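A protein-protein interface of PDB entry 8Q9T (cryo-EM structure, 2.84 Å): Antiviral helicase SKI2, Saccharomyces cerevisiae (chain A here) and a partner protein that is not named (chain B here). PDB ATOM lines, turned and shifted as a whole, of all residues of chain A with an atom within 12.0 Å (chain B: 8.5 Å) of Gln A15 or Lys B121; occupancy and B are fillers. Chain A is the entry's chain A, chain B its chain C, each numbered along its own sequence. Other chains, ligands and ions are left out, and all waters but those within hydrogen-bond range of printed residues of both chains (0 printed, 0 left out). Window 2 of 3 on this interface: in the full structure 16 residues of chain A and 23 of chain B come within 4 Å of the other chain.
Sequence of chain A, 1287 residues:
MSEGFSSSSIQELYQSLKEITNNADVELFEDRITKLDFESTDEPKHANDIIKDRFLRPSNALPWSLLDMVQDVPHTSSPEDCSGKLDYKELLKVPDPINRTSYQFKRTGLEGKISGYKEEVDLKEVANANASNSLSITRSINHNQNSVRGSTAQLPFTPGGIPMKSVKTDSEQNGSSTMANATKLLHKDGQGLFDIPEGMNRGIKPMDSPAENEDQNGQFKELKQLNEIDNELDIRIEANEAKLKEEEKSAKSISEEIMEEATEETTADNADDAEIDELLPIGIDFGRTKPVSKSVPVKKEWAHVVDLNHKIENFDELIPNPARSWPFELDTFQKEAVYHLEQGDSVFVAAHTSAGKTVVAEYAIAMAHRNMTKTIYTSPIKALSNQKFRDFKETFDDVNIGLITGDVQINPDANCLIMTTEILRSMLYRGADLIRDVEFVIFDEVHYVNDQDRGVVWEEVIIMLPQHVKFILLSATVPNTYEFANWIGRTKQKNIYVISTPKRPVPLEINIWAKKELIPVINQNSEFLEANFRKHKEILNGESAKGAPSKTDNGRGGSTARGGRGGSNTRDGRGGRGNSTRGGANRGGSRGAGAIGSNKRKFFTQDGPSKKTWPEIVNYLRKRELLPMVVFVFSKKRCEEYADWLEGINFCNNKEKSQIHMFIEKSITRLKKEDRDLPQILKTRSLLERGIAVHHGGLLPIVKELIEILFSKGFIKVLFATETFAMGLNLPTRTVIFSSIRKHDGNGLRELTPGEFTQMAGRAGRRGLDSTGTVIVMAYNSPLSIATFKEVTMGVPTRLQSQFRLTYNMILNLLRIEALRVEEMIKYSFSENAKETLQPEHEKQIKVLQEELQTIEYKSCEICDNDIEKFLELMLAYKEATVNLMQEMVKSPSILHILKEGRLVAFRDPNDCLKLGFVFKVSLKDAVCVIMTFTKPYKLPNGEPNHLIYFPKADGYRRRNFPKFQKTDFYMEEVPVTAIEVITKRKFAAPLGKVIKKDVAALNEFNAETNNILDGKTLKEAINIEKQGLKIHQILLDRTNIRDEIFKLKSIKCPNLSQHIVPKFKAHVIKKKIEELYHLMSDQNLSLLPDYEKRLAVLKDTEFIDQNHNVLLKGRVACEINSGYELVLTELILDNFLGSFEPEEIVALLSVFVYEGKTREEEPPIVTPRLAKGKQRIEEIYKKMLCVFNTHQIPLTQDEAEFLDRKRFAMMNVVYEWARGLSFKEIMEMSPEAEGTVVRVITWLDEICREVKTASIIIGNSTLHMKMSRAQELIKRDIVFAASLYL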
ATOM      1  N   GLU A  12      15.751  28.793   4.029  1.00  0.00           N
ATOM      2  CA  GLU A  12      15.561  30.137   4.559  1.00  0.00           C
ATOM      3  C   GLU A  12      16.477  31.134   3.862  1.00  0.00           C
ATOM      4  O   GLU A  12      16.145  32.312   3.735  1.00  0.00           O
ATOM      5  CB  GLU A  12      15.809  30.158   6.067  1.00  0.00           C
ATOM      6  N   LEU A  13      17.640  30.657   3.418  1.00  0.00           N
ATOM      7  CA  LEU A  13      18.561  31.510   2.676  1.00  0.00           C
ATOM      8  C   LEU A  13      18.288  31.466   1.179  1.00  0.00           C
ATOM      9  O   LEU A  13      18.469  32.475   0.487  1.00  0.00           O
ATOM     10  CB  LEU A  13      20.005  31.098   2.961  1.00  0.00           C
ATOM     11  CG  LEU A  13      20.604  31.609   4.270  1.00  0.00           C
ATOM     12  CD1 LEU A  13      21.759  30.729   4.705  1.00  0.00           C
ATOM     13  CD2 LEU A  13      21.051  33.053   4.129  1.00  0.00           C
ATOM     14  N   TYR A  14      17.854  30.316   0.663  1.00  0.00           N
ATOM     15  CA  TYR A  14      17.481  30.235  -0.742  1.00  0.00           C
ATOM     16  C   TYR A  14      16.218  31.037  -1.024  1.00  0.00           C
ATOM     17  O   TYR A  14      16.075  31.610  -2.112  1.00  0.00           O
ATOM     18  CB  TYR A  14      17.305  28.774  -1.147  1.00  0.00           C
ATOM     19  CG  TYR A  14      18.594  28.113  -1.574  1.00  0.00           C
ATOM     20  CD1 TYR A  14      19.112  28.315  -2.844  1.00  0.00           C
ATOM     21  CD2 TYR A  14      19.300  27.298  -0.702  1.00  0.00           C
ATOM     22  CE1 TYR A  14      20.289  27.717  -3.238  1.00  0.00           C
ATOM     23  CE2 TYR A  14      20.479  26.695  -1.087  1.00  0.00           C
ATOM     24  CZ  TYR A  14      20.969  26.909  -2.355  1.00  0.00           C
ATOM     25  OH  TYR A  14      22.144  26.315  -2.746  1.00  0.00           O
ATOM     26  N   GLN A  15      15.302  31.102  -0.056  1.00  0.00           N
ATOM     27  CA  GLN A  15      14.150  31.986  -0.186  1.00  0.00           C
ATOM     28  C   GLN A  15      14.590  33.440  -0.279  1.00  0.00           C
ATOM     29  O   GLN A  15      13.992  34.233  -1.014  1.00  0.00           O
ATOM     30  CB  GLN A  15      13.199  31.787   0.993  1.00  0.00           C
ATOM     31  CG  GLN A  15      12.551  30.415   1.046  1.00  0.00           C
ATOM     32  CD  GLN A  15      11.604  30.175  -0.111  1.00  0.00           C
ATOM     33  OE1 GLN A  15      11.834  29.298  -0.944  1.00  0.00           O
ATOM     34  NE2 GLN A  15      10.533  30.955  -0.170  1.00  0.00           N
ATOM     35  N   SER A  16      15.631  33.810   0.470  1.00  0.00           N
ATOM     36  CA  SER A  16      16.207  35.143   0.335  1.00  0.00           C
ATOM     37  C   SER A  16      16.824  35.340  -1.043  1.00  0.00           C
ATOM     38  O   SER A  16      16.715  36.424  -1.627  1.00  0.00           O
ATOM     39  CB  SER A  16      17.248  35.378   1.428  1.00  0.00           C
ATOM     40  OG  SER A  16      16.693  35.167   2.713  1.00  0.00           O
ATOM     41  N   LEU A  17      17.488  34.309  -1.574  1.00  0.00           N
ATOM     42  CA  LEU A  17      18.052  34.414  -2.916  1.00  0.00           C
ATOM     43  C   LEU A  17      16.975  34.563  -3.980  1.00  0.00           C
ATOM     44  O   LEU A  17      17.237  35.137  -5.043  1.00  0.00           O
ATOM     45  CB  LEU A  17      18.918  33.199  -3.239  1.00  0.00           C
ATOM     46  CG  LEU A  17      20.234  33.011  -2.498  1.00  0.00           C
ATOM     47  CD1 LEU A  17      20.849  31.689  -2.902  1.00  0.00           C
ATOM     48  CD2 LEU A  17      21.169  34.153  -2.831  1.00  0.00           C
ATOM     49  N   LYS A  18      15.773  34.040  -3.728  1.00  0.00           N
ATOM     50  CA  LYS A  18      14.710  34.147  -4.725  1.00  0.00           C
ATOM     51  C   LYS A  18      14.375  35.603  -5.019  1.00  0.00           C
ATOM     52  O   LYS A  18      14.183  35.982  -6.180  1.00  0.00           O
ATOM     53  CB  LYS A  18      13.466  33.394  -4.260  1.00  0.00           C
ATOM     54  CG  LYS A  18      13.598  31.883  -4.337  1.00  0.00           C
ATOM     55  CD  LYS A  18      13.805  31.414  -5.767  1.00  0.00           C
ATOM     56  CE  LYS A  18      12.503  31.384  -6.537  1.00  0.00           C
ATOM     57  NZ  LYS A  18      12.667  30.723  -7.856  1.00  0.00           N
ATOM     58  N   GLU A  19      14.306  36.434  -3.985  1.00  0.00           N
ATOM     59  CA  GLU A  19      14.069  37.860  -4.167  1.00  0.00           C
ATOM     60  C   GLU A  19      15.325  38.553  -4.687  1.00  0.00           C
ATOM     61  O   GLU A  19      15.343  39.075  -5.801  1.00  0.00           O
ATOM     62  CB  GLU A  19      13.619  38.501  -2.853  1.00  0.00           C
ATOM     63  N   SER B  90      20.053  31.862  -8.318  1.00  0.00           N
ATOM     64  CA  SER B  90      18.996  32.170  -7.359  1.00  0.00           C
ATOM     65  C   SER B  90      18.029  31.003  -7.197  1.00  0.00           C
ATOM     66  O   SER B  90      17.471  30.812  -6.112  1.00  0.00           O
ATOM     67  CB  SER B  90      18.245  33.430  -7.784  1.00  0.00           C
ATOM     68  OG  SER B  90      17.421  33.180  -8.905  1.00  0.00           O
ATOM     69  N   GLY B  91      17.820  30.219  -8.250  1.00  0.00           N
ATOM     70  CA  GLY B  91      16.999  29.030  -8.147  1.00  0.00           C
ATOM     71  C   GLY B  91      15.811  29.005  -9.084  1.00  0.00           C
ATOM     72  O   GLY B  91      14.820  28.320  -8.818  1.00  0.00           O
ATOM     73  N   ASP B  92      15.897  29.743 -10.185  1.00  0.00           N
ATOM     74  CA  ASP B  92      14.805  29.826 -11.142  1.00  0.00           C
ATOM     75  C   ASP B  92      14.978  28.799 -12.251  1.00  0.00           C
ATOM     76  O   ASP B  92      16.088  28.353 -12.547  1.00  0.00           O
ATOM     77  CB  ASP B  92      14.721  31.229 -11.743  1.00  0.00           C
ATOM     78  CG  ASP B  92      14.455  32.291 -10.701  1.00  0.00           C
ATOM     79  OD1 ASP B  92      14.080  31.930  -9.568  1.00  0.00           O
ATOM     80  OD2 ASP B  92      14.619  33.488 -11.013  1.00  0.00           O
ATOM     81  N   LEU B 115       5.770  27.662 -16.300  1.00  0.00           N
ATOM     82  CA  LEU B 115       5.498  27.266 -14.927  1.00  0.00           C
ATOM     83  C   LEU B 115       4.435  28.174 -14.325  1.00  0.00           C
ATOM     84  O   LEU B 115       4.422  29.382 -14.573  1.00  0.00           O
ATOM     85  CB  LEU B 115       6.771  27.322 -14.082  1.00  0.00           C
ATOM     86  CG  LEU B 115       7.821  26.245 -14.360  1.00  0.00           C
ATOM     87  CD1 LEU B 115       8.953  26.336 -13.356  1.00  0.00           C
ATOM     88  CD2 LEU B 115       7.196  24.864 -14.342  1.00  0.00           C
ATOM     89  N   ASP B 116       3.545  27.585 -13.530  1.00  0.00           N
ATOM     90  CA  ASP B 116       2.466  28.336 -12.903  1.00  0.00           C
ATOM     91  C   ASP B 116       3.022  29.153 -11.738  1.00  0.00           C
ATOM     92  O   ASP B 116       4.233  29.211 -11.508  1.00  0.00           O
ATOM     93  CB  ASP B 116       1.349  27.392 -12.465  1.00  0.00           C
ATOM     94  CG  ASP B 116       1.853  26.255 -11.602  1.00  0.00           C
ATOM     95  OD1 ASP B 116       2.582  25.389 -12.129  1.00  0.00           O
ATOM     96  OD2 ASP B 116       1.517  26.224 -10.399  1.00  0.00           O
ATOM     97  N   SER B 117       2.134  29.805 -10.985  1.00  0.00           N
ATOM     98  CA  SER B 117       2.585  30.682  -9.910  1.00  0.00           C
ATOM     99  C   SER B 117       3.097  29.889  -8.715  1.00  0.00           C
ATOM    100  O   SER B 117       4.083  30.281  -8.081  1.00  0.00           O
ATOM    101  CB  SER B 117       1.455  31.619  -9.486  1.00  0.00           C
ATOM    102  OG  SER B 117       1.902  32.543  -8.511  1.00  0.00           O
ATOM    103  N   ASP B 118       2.442  28.773  -8.387  1.00  0.00           N
ATOM    104  CA  ASP B 118       2.873  27.971  -7.249  1.00  0.00           C
ATOM    105  C   ASP B 118       4.161  27.213  -7.531  1.00  0.00           C
ATOM    106  O   ASP B 118       4.853  26.816  -6.587  1.00  0.00           O
ATOM    107  CB  ASP B 118       1.773  26.989  -6.846  1.00  0.00           C
ATOM    108  CG  ASP B 118       0.741  27.617  -5.935  1.00  0.00           C
ATOM    109  OD1 ASP B 118       1.131  28.403  -5.046  1.00  0.00           O
ATOM    110  OD2 ASP B 118      -0.461  27.328  -6.108  1.00  0.00           O
ATOM    111  N   MET B 119       4.497  27.001  -8.799  1.00  0.00           N
ATOM    112  CA  MET B 119       5.721  26.313  -9.176  1.00  0.00           C
ATOM    113  C   MET B 119       6.913  27.251  -9.281  1.00  0.00           C
ATOM    114  O   MET B 119       8.030  26.785  -9.528  1.00  0.00           O
ATOM    115  CB  MET B 119       5.519  25.581 -10.504  1.00  0.00           C
ATOM    116  CG  MET B 119       6.330  24.312 -10.636  1.00  0.00           C
ATOM    117  SD  MET B 119       5.616  22.958  -9.693  1.00  0.00           S
ATOM    118  CE  MET B 119       7.094  22.046  -9.287  1.00  0.00           C
ATOM    119  N   LYS B 120       6.709  28.552  -9.104  1.00  0.00           N
ATOM    120  CA  LYS B 120       7.788  29.526  -9.169  1.00  0.00           C
ATOM    121  C   LYS B 120       8.382  29.842  -7.803  1.00  0.00           C
ATOM    122  O   LYS B 120       9.288  30.676  -7.718  1.00  0.00           O
ATOM    123  CB  LYS B 120       7.294  30.816  -9.827  1.00  0.00           C
ATOM    124  CG  LYS B 120       7.106  30.707 -11.329  1.00  0.00           C
ATOM    125  CD  LYS B 120       6.580  32.006 -11.914  1.00  0.00           C
ATOM    126  CE  LYS B 120       6.311  31.868 -13.402  1.00  0.00           C
ATOM    127  NZ  LYS B 120       7.565  31.649 -14.172  1.00  0.00           N
ATOM    128  N   LYS B 121       7.898  29.206  -6.742  1.00  0.00           N
ATOM    129  CA  LYS B 121       8.423  29.414  -5.402  1.00  0.00           C
ATOM    130  C   LYS B 121       9.482  28.394  -5.014  1.00  0.00           C
ATOM    131  O   LYS B 121       9.982  28.441  -3.887  1.00  0.00           O
ATOM    132  CB  LYS B 121       7.285  29.381  -4.378  1.00  0.00           C
ATOM    133  CG  LYS B 121       6.266  30.496  -4.534  1.00  0.00           C
ATOM    134  CD  LYS B 121       5.212  30.423  -3.444  1.00  0.00           C
ATOM    135  CE  LYS B 121       4.203  31.553  -3.565  1.00  0.00           C
ATOM    136  NZ  LYS B 121       3.283  31.357  -4.718  1.00  0.00           N
ATOM    137  N   HIS B 122       9.832  27.476  -5.908  1.00  0.00           N
ATOM    138  CA  HIS B 122      10.812  26.443  -5.614  1.00  0.00           C
ATOM    139  C   HIS B 122      12.181  26.831  -6.152  1.00  0.00           C
ATOM    140  O   HIS B 122      12.300  27.519  -7.169  1.00  0.00           O
ATOM    141  CB  HIS B 122      10.385  25.102  -6.212  1.00  0.00           C
ATOM    142  CG  HIS B 122       9.179  24.505  -5.559  1.00  0.00           C
ATOM    143  ND1 HIS B 122       8.034  24.193  -6.257  1.00  0.00           N
ATOM    144  CD2 HIS B 122       8.941  24.160  -4.272  1.00  0.00           C
ATOM    145  CE1 HIS B 122       7.141  23.682  -5.429  1.00  0.00           C
ATOM    146  NE2 HIS B 122       7.667  23.651  -4.217  1.00  0.00           N
ATOM    147  N   SER B 123      13.219  26.376  -5.456  1.00  0.00           N
ATOM    148  CA  SER B 123      14.599  26.583  -5.870  1.00  0.00           C
ATOM    149  C   SER B 123      15.107  25.305  -6.520  1.00  0.00           C
ATOM    150  O   SER B 123      15.217  24.271  -5.856  1.00  0.00           O
ATOM    151  CB  SER B 123      15.475  26.964  -4.677  1.00  0.00           C
ATOM    152  OG  SER B 123      14.883  28.001  -3.919  1.00  0.00           O
ATOM    153  N   PHE B 124      15.421  25.374  -7.806  1.00  0.00           N
ATOM    154  CA  PHE B 124      15.858  24.208  -8.557  1.00  0.00           C
ATOM    155  C   PHE B 124      17.375  24.191  -8.676  1.00  0.00           C
ATOM    156  O   PHE B 124      18.028  25.235  -8.641  1.00  0.00           O
ATOM    157  CB  PHE B 124      15.220  24.188  -9.947  1.00  0.00           C
ATOM    158  CG  PHE B 124      13.722  24.141  -9.921  1.00  0.00           C
ATOM    159  CD1 PHE B 124      13.056  22.943  -9.735  1.00  0.00           C
ATOM    160  CD2 PHE B 124      12.977  25.295 -10.073  1.00  0.00           C
ATOM    161  CE1 PHE B 124      11.680  22.898  -9.704  1.00  0.00           C
ATOM    162  CE2 PHE B 124      11.599  25.255 -10.045  1.00  0.00           C
ATOM    163  CZ  PHE B 124      10.952  24.055  -9.860  1.00  0.00           C
ATOM    164  N   ASP B 145      15.351  19.481  -6.528  1.00  0.00           N
ATOM    165  CA  ASP B 145      15.106  20.583  -5.614  1.00  0.00           C
ATOM    166  C   ASP B 145      16.181  20.596  -4.534  1.00  0.00           C
ATOM    167  O   ASP B 145      16.821  19.580  -4.253  1.00  0.00           O
ATOM    168  CB  ASP B 145      13.709  20.447  -4.994  1.00  0.00           C
ATOM    169  CG  ASP B 145      13.310  21.640  -4.157  1.00  0.00           C
ATOM    170  OD1 ASP B 145      14.070  22.623  -4.107  1.00  0.00           O
ATOM    171  OD2 ASP B 145      12.223  21.593  -3.547  1.00  0.00           O
ATOM    172  N   VAL B 146      16.388  21.770  -3.933  1.00  0.00           N
ATOM    173  CA  VAL B 146      17.340  21.863  -2.833  1.00  0.00           C
ATOM    174  C   VAL B 146      16.841  21.122  -1.601  1.00  0.00           C
ATOM    175  O   VAL B 146      17.627  20.850  -0.687  1.00  0.00           O
ATOM    176  CB  VAL B 146      17.649  23.331  -2.487  1.00  0.00           C
ATOM    177  CG1 VAL B 146      18.112  24.081  -3.722  1.00  0.00           C
ATOM    178  CG2 VAL B 146      16.436  24.001  -1.867  1.00  0.00           C
ATOM    179  N   TYR B 151      10.890  16.354  -9.725  1.00  0.00           N
ATOM    180  CA  TYR B 151       9.629  16.672 -10.379  1.00  0.00           C
ATOM    181  C   TYR B 151       9.627  16.133 -11.802  1.00  0.00           C
ATOM    182  O   TYR B 151      10.648  16.178 -12.494  1.00  0.00           O
ATOM    183  CB  TYR B 151       9.380  18.181 -10.400  1.00  0.00           C
ATOM    184  CG  TYR B 151       9.381  18.822  -9.034  1.00  0.00           C
ATOM    185  CD1 TYR B 151      10.553  19.307  -8.476  1.00  0.00           C
ATOM    186  CD2 TYR B 151       8.212  18.937  -8.303  1.00  0.00           C
ATOM    187  CE1 TYR B 151      10.559  19.890  -7.229  1.00  0.00           C
ATOM    188  CE2 TYR B 151       8.207  19.519  -7.054  1.00  0.00           C
ATOM    189  CZ  TYR B 151       9.383  19.994  -6.522  1.00  0.00           C
ATOM    190  OH  TYR B 151       9.383  20.575  -5.278  1.00  0.00           O
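The side-chain amino group (NZ) of Lys A18 lies within salt-bridge range of the side-chain carboxylate (OD1) of Asp B92, at 2.5 Å.
The side-chain amino group (NZ) of Lys A18 is in hydrogen-bond range of the backbone carbonyl oxygen (O) of Lys B120 (3.4 Å).
The side-chain amino group of Lys A18 lies within hydrogen-bond range of the backbone carbonyl oxygen of His B122 (3.3 Å).
The backbone carbonyl oxygen (O) of Gly B91 lies within hydrogen-bond range of the side-chain amino group (NZ) of Lys A18, 3.4 Å away.
The backbone carbonyl oxygen (O) of Ser B123 sits close to the side-chain carboxylate (OD1) of Asp B145 (2.7 Å).
O of Ser B123 is in hydrogen-bond range of N of Val B146 (3.4 Å).
The backbone carbonyl oxygen of Gly B91 sits at hydrogen-bond distance from the backbone NH of Phe B124 (3.2 Å).
The side-chain amino group (NZ) of Lys B121 lies within salt-bridge range of the side-chain carboxylate (OD1) of Asp B118, at 3.7 Å.
Among the printed residues, merely in contact across the chains: Leu A17 with Ser B90, Gln A15 with Lys B121, Lys A18 with Ser B90 and Tyr A14 with Ser B123.
Of the printed residues of chain B, Gln A15 touches Lys B121.
Ser A16 touches none of the printed residues of chain B.
Printed residues of chain B within 4 Å of Leu A17: Ser B90.
Of the printed residues of chain A, Ser B90 touches Leu A17 (3.4 Å) and Lys A18 (3.7 Å).
Of the printed residues of chain A, Asp B92 touches Lys A18.
Met B119 touches none of the printed residues of chain A.
Of chain A, only Gln A15 comes within 4 Å of Lys B121.
Ser B123 touches one residue of chain A.
Val B146 touches none of the printed residues of chain A.
The nearest printed residue of chain A that does not touch Ser B90 is Tyr A14 (4.3 Å).
Of the 16 printed residues of chain B, 7 touch a printed residue of chain A.
Printed residues of chain A that touch a printed residue of chain B: Tyr A14, Gln A15, Leu A17 and Lys A18.
Hydrophobic or aromatic side chains of chain A that line the printed part of chain B: Tyr A14.
Among the printed residues, 8 pairs touch across the chains.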
